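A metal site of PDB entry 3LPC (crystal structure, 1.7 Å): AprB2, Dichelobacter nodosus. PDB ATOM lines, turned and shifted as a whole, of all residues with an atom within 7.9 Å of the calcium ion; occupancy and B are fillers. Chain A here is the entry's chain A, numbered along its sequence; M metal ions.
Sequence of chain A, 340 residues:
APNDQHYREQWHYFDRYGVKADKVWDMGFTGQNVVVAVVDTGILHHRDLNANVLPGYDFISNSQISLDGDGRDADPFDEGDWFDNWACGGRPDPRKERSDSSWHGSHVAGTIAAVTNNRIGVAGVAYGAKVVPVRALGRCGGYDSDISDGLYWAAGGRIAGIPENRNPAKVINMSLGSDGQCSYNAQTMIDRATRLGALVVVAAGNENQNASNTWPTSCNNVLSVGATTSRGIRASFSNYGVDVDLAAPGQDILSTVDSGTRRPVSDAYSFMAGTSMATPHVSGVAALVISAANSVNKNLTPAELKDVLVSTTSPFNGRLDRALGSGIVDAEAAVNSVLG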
ATOM      1  N   PRO A   2     -19.649 -10.769   4.561  1.00  0.00           N
ATOM      2  CA  PRO A   2     -20.847  -9.993   4.239  1.00  0.00           C
ATOM      3  C   PRO A   2     -21.687  -9.679   5.460  1.00  0.00           C
ATOM      4  O   PRO A   2     -21.592 -10.371   6.458  1.00  0.00           O
ATOM      5  CB  PRO A   2     -21.636 -10.915   3.308  1.00  0.00           C
ATOM      6  CG  PRO A   2     -21.094 -12.287   3.561  1.00  0.00           C
ATOM      7  CD  PRO A   2     -19.677 -12.119   3.975  1.00  0.00           C
ATOM      8  N   ASN A   3     -22.546  -8.666   5.355  1.00  0.00           N
ATOM      9  CA  ASN A   3     -23.348  -8.201   6.483  1.00  0.00           C
ATOM     10  C   ASN A   3     -24.653  -8.952   6.706  1.00  0.00           C
ATOM     11  O   ASN A   3     -25.423  -8.642   7.619  1.00  0.00           O
ATOM     12  CB  ASN A   3     -23.603  -6.669   6.392  1.00  0.00           C
ATOM     13  CG  ASN A   3     -24.507  -6.278   5.228  1.00  0.00           C
ATOM     14  OD1 ASN A   3     -25.315  -7.077   4.747  1.00  0.00           O
ATOM     15  ND2 ASN A   3     -24.389  -5.025   4.771  1.00  0.00           N
ATOM     16  N   ASP A   4     -24.934  -9.961   5.882  1.00  0.00           N
ATOM     17  CA  ASP A   4     -26.225 -10.624   5.946  1.00  0.00           C
ATOM     18  C   ASP A   4     -26.556 -11.268   7.287  1.00  0.00           C
ATOM     19  O   ASP A   4     -25.702 -11.893   7.928  1.00  0.00           O
ATOM     20  CB  ASP A   4     -26.380 -11.612   4.805  1.00  0.00           C
ATOM     21  CG  ASP A   4     -26.081 -10.969   3.491  1.00  0.00           C
ATOM     22  OD1 ASP A   4     -27.038 -10.592   2.789  1.00  0.00           O
ATOM     23  OD2 ASP A   4     -24.889 -10.786   3.187  1.00  0.00           O
ATOM     24  N   GLN A   5     -27.806 -11.061   7.722  1.00  0.00           N
ATOM     25  CA  GLN A   5     -28.273 -11.471   9.044  1.00  0.00           C
ATOM     26  C   GLN A   5     -27.949 -12.922   9.423  1.00  0.00           C
ATOM     27  O   GLN A   5     -27.554 -13.182  10.567  1.00  0.00           O
ATOM     28  CB  GLN A   5     -29.770 -11.185   9.185  1.00  0.00           C
ATOM     29  CG  GLN A   5     -30.221 -11.103  10.622  1.00  0.00           C
ATOM     30  CD  GLN A   5     -31.498 -10.289  10.825  1.00  0.00           C
ATOM     31  OE1 GLN A   5     -32.371 -10.238   9.957  1.00  0.00           O
ATOM     32  NE2 GLN A   5     -31.597  -9.668  11.987  1.00  0.00           N
ATOM     33  N   HIS A   6     -28.101 -13.851   8.478  1.00  0.00           N
ATOM     34  CA  HIS A   6     -27.894 -15.266   8.787  1.00  0.00           C
ATOM     35  C   HIS A   6     -26.668 -15.876   8.089  1.00  0.00           C
ATOM     36  O   HIS A   6     -26.546 -17.110   8.034  1.00  0.00           O
ATOM     37  CB  HIS A   6     -29.156 -16.072   8.494  1.00  0.00           C
ATOM     38  CG  HIS A   6     -30.308 -15.662   9.367  1.00  0.00           C
ATOM     39  ND1 HIS A   6     -30.469 -16.129  10.651  1.00  0.00           N
ATOM     40  CD2 HIS A   6     -31.305 -14.774   9.156  1.00  0.00           C
ATOM     41  CE1 HIS A   6     -31.538 -15.564  11.191  1.00  0.00           C
ATOM     42  NE2 HIS A   6     -32.050 -14.724  10.307  1.00  0.00           N
ATOM     43  N   TYR A   7     -25.773 -15.034   7.584  1.00  0.00           N
ATOM     44  CA  TYR A   7     -24.531 -15.544   6.997  1.00  0.00           C
ATOM     45  C   TYR A   7     -23.771 -16.504   7.916  1.00  0.00           C
ATOM     46  O   TYR A   7     -23.279 -17.531   7.449  1.00  0.00           O
ATOM     47  CB  TYR A   7     -23.616 -14.421   6.516  1.00  0.00           C
ATOM     48  CG  TYR A   7     -22.220 -14.885   6.155  1.00  0.00           C
ATOM     49  CD1 TYR A   7     -21.998 -15.666   5.015  1.00  0.00           C
ATOM     50  CD2 TYR A   7     -21.118 -14.533   6.936  1.00  0.00           C
ATOM     51  CE1 TYR A   7     -20.714 -16.081   4.673  1.00  0.00           C
ATOM     52  CE2 TYR A   7     -19.832 -14.955   6.615  1.00  0.00           C
ATOM     53  CZ  TYR A   7     -19.632 -15.736   5.484  1.00  0.00           C
ATOM     54  OH  TYR A   7     -18.363 -16.169   5.143  1.00  0.00           O
ATOM     55  N   GLN A  10     -24.375 -20.127   7.579  1.00  0.00           N
ATOM     56  CA  GLN A  10     -23.971 -20.778   6.336  1.00  0.00           C
ATOM     57  C   GLN A  10     -22.560 -21.326   6.406  1.00  0.00           C
ATOM     58  O   GLN A  10     -21.675 -20.891   5.638  1.00  0.00           O
ATOM     59  CB  GLN A  10     -24.187 -19.811   5.144  1.00  0.00           C
ATOM     60  CG  GLN A  10     -25.655 -19.420   5.016  1.00  0.00           C
ATOM     61  CD  GLN A  10     -25.922 -18.485   3.854  1.00  0.00           C
ATOM     62  OE1 GLN A  10     -25.454 -17.343   3.840  1.00  0.00           O
ATOM     63  NE2 GLN A  10     -26.685 -18.979   2.854  1.00  0.00           N
ATOM     64  N   HIS A  46     -38.640 -13.282  -4.120  1.00  0.00           N
ATOM     65  CA  HIS A  46     -38.119 -13.185  -2.753  1.00  0.00           C
ATOM     66  C   HIS A  46     -37.213 -11.987  -2.678  1.00  0.00           C
ATOM     67  O   HIS A  46     -36.386 -11.752  -3.570  1.00  0.00           O
ATOM     68  CB  HIS A  46     -37.352 -14.493  -2.503  1.00  0.00           C
ATOM     69  CG  HIS A  46     -36.950 -14.749  -1.078  1.00  0.00           C
ATOM     70  ND1 HIS A  46     -36.136 -13.897  -0.371  1.00  0.00           N
ATOM     71  CD2 HIS A  46     -37.174 -15.811  -0.284  1.00  0.00           C
ATOM     72  CE1 HIS A  46     -35.907 -14.410   0.828  1.00  0.00           C
ATOM     73  NE2 HIS A  46     -36.518 -15.580   0.908  1.00  0.00           N
ATOM     74  N   ARG A  47     -37.346 -11.204  -1.613  1.00  0.00           N
ATOM     75  CA  ARG A  47     -36.570  -9.990  -1.437  1.00  0.00           C
ATOM     76  C   ARG A  47     -35.051 -10.233  -1.400  1.00  0.00           C
ATOM     77  O   ARG A  47     -34.258  -9.343  -1.754  1.00  0.00           O
ATOM     78  CB  ARG A  47     -37.042  -9.314  -0.170  1.00  0.00           C
ATOM     79  CG  ARG A  47     -36.647  -7.911  -0.052  1.00  0.00           C
ATOM     80  CD  ARG A  47     -37.294  -7.378   1.189  1.00  0.00           C
ATOM     81  NE  ARG A  47     -36.840  -6.030   1.446  1.00  0.00           N
ATOM     82  CZ  ARG A  47     -37.356  -5.258   2.390  1.00  0.00           C
ATOM     83  NH1 ARG A  47     -38.339  -5.719   3.155  1.00  0.00           N
ATOM     84  NH2 ARG A  47     -36.879  -4.022   2.558  1.00  0.00           N
ATOM     85  N   ASP A  48     -34.650 -11.430  -0.990  1.00  0.00           N
ATOM     86  CA  ASP A  48     -33.253 -11.789  -0.969  1.00  0.00           C
ATOM     87  C   ASP A  48     -32.793 -12.508  -2.253  1.00  0.00           C
ATOM     88  O   ASP A  48     -31.658 -12.989  -2.285  1.00  0.00           O
ATOM     89  CB  ASP A  48     -32.891 -12.600   0.286  1.00  0.00           C
ATOM     90  CG  ASP A  48     -31.550 -12.189   0.883  1.00  0.00           C
ATOM     91  OD1 ASP A  48     -31.138 -11.020   0.672  1.00  0.00           O
ATOM     92  OD2 ASP A  48     -30.906 -12.998   1.581  1.00  0.00           O
ATOM     93  N   LEU A  49     -33.668 -12.566  -3.272  1.00  0.00           N
ATOM     94  CA  LEU A  49     -33.294 -13.086  -4.609  1.00  0.00           C
ATOM     95  C   LEU A  49     -33.428 -12.059  -5.732  1.00  0.00           C
ATOM     96  O   LEU A  49     -32.613 -12.049  -6.674  1.00  0.00           O
ATOM     97  CB  LEU A  49     -34.147 -14.296  -4.992  1.00  0.00           C
ATOM     98  CG  LEU A  49     -33.929 -15.514  -4.118  1.00  0.00           C
ATOM     99  CD1 LEU A  49     -34.943 -16.578  -4.494  1.00  0.00           C
ATOM    100  CD2 LEU A  49     -32.497 -15.986  -4.326  1.00  0.00           C
ATOM    101  N   ALA A 114     -27.879 -15.612  -3.866  1.00  0.00           N
ATOM    102  CA  ALA A 114     -28.720 -14.813  -2.963  1.00  0.00           C
ATOM    103  C   ALA A 114     -28.080 -13.431  -2.891  1.00  0.00           C
ATOM    104  O   ALA A 114     -26.853 -13.302  -2.956  1.00  0.00           O
ATOM    105  CB  ALA A 114     -28.794 -15.437  -1.569  1.00  0.00           C
ATOM    106  N   VAL A 115     -28.924 -12.407  -2.784  1.00  0.00           N
ATOM    107  CA  VAL A 115     -28.445 -11.037  -2.719  1.00  0.00           C
ATOM    108  C   VAL A 115     -27.665 -10.901  -1.422  1.00  0.00           C
ATOM    109  O   VAL A 115     -28.158 -11.255  -0.358  1.00  0.00           O
ATOM    110  CB  VAL A 115     -29.616 -10.022  -2.761  1.00  0.00           C
ATOM    111  CG1 VAL A 115     -29.067  -8.591  -2.658  1.00  0.00           C
ATOM    112  CG2 VAL A 115     -30.464 -10.201  -4.048  1.00  0.00           C
ATOM    113  N   THR A 116     -26.446 -10.388  -1.515  1.00  0.00           N
ATOM    114  CA  THR A 116     -25.515 -10.424  -0.394  1.00  0.00           C
ATOM    115  C   THR A 116     -25.100  -8.995  -0.046  1.00  0.00           C
ATOM    116  O   THR A 116     -25.093  -8.104  -0.927  1.00  0.00           O
ATOM    117  CB  THR A 116     -24.332 -11.318  -0.776  1.00  0.00           C
ATOM    118  OG1 THR A 116     -24.847 -12.609  -1.061  1.00  0.00           O
ATOM    119  CG2 THR A 116     -23.283 -11.435   0.310  1.00  0.00           C
ATOM    120  N   ASN A 117     -24.784  -8.774   1.228  1.00  0.00           N
ATOM    121  CA  ASN A 117     -24.425  -7.441   1.732  1.00  0.00           C
ATOM    122  C   ASN A 117     -25.627  -6.476   1.684  1.00  0.00           C
ATOM    123  O   ASN A 117     -25.444  -5.250   1.565  1.00  0.00           O
ATOM    124  CB  ASN A 117     -23.239  -6.849   0.966  1.00  0.00           C
ATOM    125  CG  ASN A 117     -21.903  -7.271   1.533  1.00  0.00           C
ATOM    126  OD1 ASN A 117     -21.717  -7.264   2.760  1.00  0.00           O
ATOM    127  ND2 ASN A 117     -20.943  -7.608   0.652  1.00  0.00           N
ATOM    128  N   ASN A 118     -26.836  -7.032   1.751  1.00  0.00           N
ATOM    129  CA  ASN A 118     -28.077  -6.242   1.798  1.00  0.00           C
ATOM    130  C   ASN A 118     -28.786  -6.362   3.159  1.00  0.00           C
ATOM    131  O   ASN A 118     -30.010  -6.134   3.291  1.00  0.00           O
ATOM    132  CB  ASN A 118     -29.010  -6.592   0.633  1.00  0.00           C
ATOM    133  CG  ASN A 118     -29.622  -7.988   0.785  1.00  0.00           C
ATOM    134  OD1 ASN A 118     -29.029  -8.874   1.426  1.00  0.00           O
ATOM    135  ND2 ASN A 118     -30.820  -8.190   0.235  1.00  0.00           N
ATOM    136  N   ARG A 119     -28.017  -6.747   4.174  1.00  0.00           N
ATOM    137  CA  ARG A 119     -28.473  -6.862   5.579  1.00  0.00           C
ATOM    138  C   ARG A 119     -29.399  -8.049   5.854  1.00  0.00           C
ATOM    139  O   ARG A 119     -29.196  -8.759   6.829  1.00  0.00           O
ATOM    140  CB  ARG A 119     -29.061  -5.547   6.134  1.00  0.00           C
ATOM    141  N   ILE A 120     -30.389  -8.287   5.008  1.00  0.00           N
ATOM    142  CA  ILE A 120     -31.373  -9.310   5.304  1.00  0.00           C
ATOM    143  C   ILE A 120     -30.882 -10.679   4.869  1.00  0.00           C
ATOM    144  O   ILE A 120     -30.009 -10.790   3.982  1.00  0.00           O
ATOM    145  CB  ILE A 120     -32.762  -9.048   4.639  1.00  0.00           C
ATOM    146  CG1 ILE A 120     -32.636  -8.940   3.116  1.00  0.00           C
ATOM    147  CG2 ILE A 120     -33.427  -7.784   5.265  1.00  0.00           C
ATOM    148  CD1 ILE A 120     -33.947  -9.043   2.359  1.00  0.00           C
ATOM    149  N   GLY A 121     -31.407 -11.713   5.534  1.00  0.00           N
ATOM    150  CA  GLY A 121     -31.346 -13.089   5.016  1.00  0.00           C
ATOM    151  C   GLY A 121     -29.962 -13.670   4.927  1.00  0.00           C
ATOM    152  O   GLY A 121     -29.229 -13.707   5.917  1.00  0.00           O
ATOM    153  N   VAL A 122     -29.613 -14.162   3.736  1.00  0.00           N
ATOM    154  CA  VAL A 122     -28.434 -14.983   3.599  1.00  0.00           C
ATOM    155  C   VAL A 122     -27.479 -14.415   2.540  1.00  0.00           C
ATOM    156  O   VAL A 122     -27.742 -13.361   1.971  1.00  0.00           O
ATOM    157  CB  VAL A 122     -28.835 -16.418   3.243  1.00  0.00           C
ATOM    158  CG1 VAL A 122     -29.543 -17.107   4.427  1.00  0.00           C
ATOM    159  CG2 VAL A 122     -29.728 -16.435   1.988  1.00  0.00           C
ATOM    160  N   ALA A 123     -26.387 -15.124   2.286  1.00  0.00           N
ATOM    161  CA  ALA A 123     -25.468 -14.800   1.209  1.00  0.00           C
ATOM    162  C   ALA A 123     -25.519 -15.866   0.112  1.00  0.00           C
ATOM    163  O   ALA A 123     -26.056 -16.962   0.319  1.00  0.00           O
ATOM    164  CB  ALA A 123     -24.041 -14.679   1.749  1.00  0.00           C
ATOM    165  N   GLY A 124     -24.950 -15.531  -1.036  1.00  0.00           N
ATOM    166  CA  GLY A 124     -24.803 -16.479  -2.144  1.00  0.00           C
ATOM    167  C   GLY A 124     -23.327 -16.719  -2.462  1.00  0.00           C
ATOM    168  O   GLY A 124     -22.509 -15.820  -2.293  1.00  0.00           O
ATOM    169  N   THR A 256     -32.800 -19.608   0.596  1.00  0.00           N
ATOM    170  CA  THR A 256     -34.015 -18.822   0.413  1.00  0.00           C
ATOM    171  C   THR A 256     -35.212 -19.669  -0.024  1.00  0.00           C
ATOM    172  O   THR A 256     -35.155 -20.294  -1.057  1.00  0.00           O
ATOM    173  CB  THR A 256     -33.774 -17.744  -0.684  1.00  0.00           C
ATOM    174  OG1 THR A 256     -33.042 -18.339  -1.764  1.00  0.00           O
ATOM    175  CG2 THR A 256     -32.952 -16.583  -0.127  1.00  0.00           C
ATOM    176  N   TYR A 269     -36.408 -18.595   5.048  1.00  0.00           N
ATOM    177  CA  TYR A 269     -35.088 -19.203   4.898  1.00  0.00           C
ATOM    178  C   TYR A 269     -35.161 -20.551   5.588  1.00  0.00           C
ATOM    179  O   TYR A 269     -35.694 -20.641   6.684  1.00  0.00           O
ATOM    180  CB  TYR A 269     -34.006 -18.330   5.547  1.00  0.00           C
ATOM    181  CG  TYR A 269     -34.051 -16.926   5.047  1.00  0.00           C
ATOM    182  CD1 TYR A 269     -33.374 -16.561   3.892  1.00  0.00           C
ATOM    183  CD2 TYR A 269     -34.839 -15.955   5.685  1.00  0.00           C
ATOM    184  CE1 TYR A 269     -33.455 -15.242   3.388  1.00  0.00           C
ATOM    185  CE2 TYR A 269     -34.918 -14.642   5.211  1.00  0.00           C
ATOM    186  CZ  TYR A 269     -34.237 -14.308   4.059  1.00  0.00           C
ATOM    187  OH  TYR A 269     -34.315 -13.042   3.571  1.00  0.00           O
HETATM  188 CA    CA M   1     -28.980 -11.271   1.842  1.00  0.00          CA
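OD1 of Asp 4 is bound to the calcium ion (2.3 Å). The backbone carbonyl oxygen (O) of Val 115 is bound to the calcium ion (2.3 Å). The calcium ion is bound by the backbone carbonyl oxygen (O) of Ile 120 (2.4 Å). O of Val 122 binds the calcium ion. The side-chain amide oxygen (OD1) of Asn 118 is bound to the calcium ion, at 2.4 Å. The side-chain carboxylate (OD1) of Asp 48 binds the calcium ion (2.5 Å). The calcium ion is bound by OD2 of Asp 48.
A ring nitrogen (ND1) of His 46 lies within hydrogen-bond range of the backbone NH of Asp 48 (2.9 Å). N of Asn 118 sits at hydrogen-bond distance from OD1 of Asn 3, 3.4 Å away. OD2 of Asp 4 sits at hydrogen-bond distance from N of Asn 117 (2.8 Å).
Of the 24 residues printed, 6 come within 4 Å of the calcium ion. Along chain A the residues within 4 Å of the calcium ion span positions 4 to 122.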
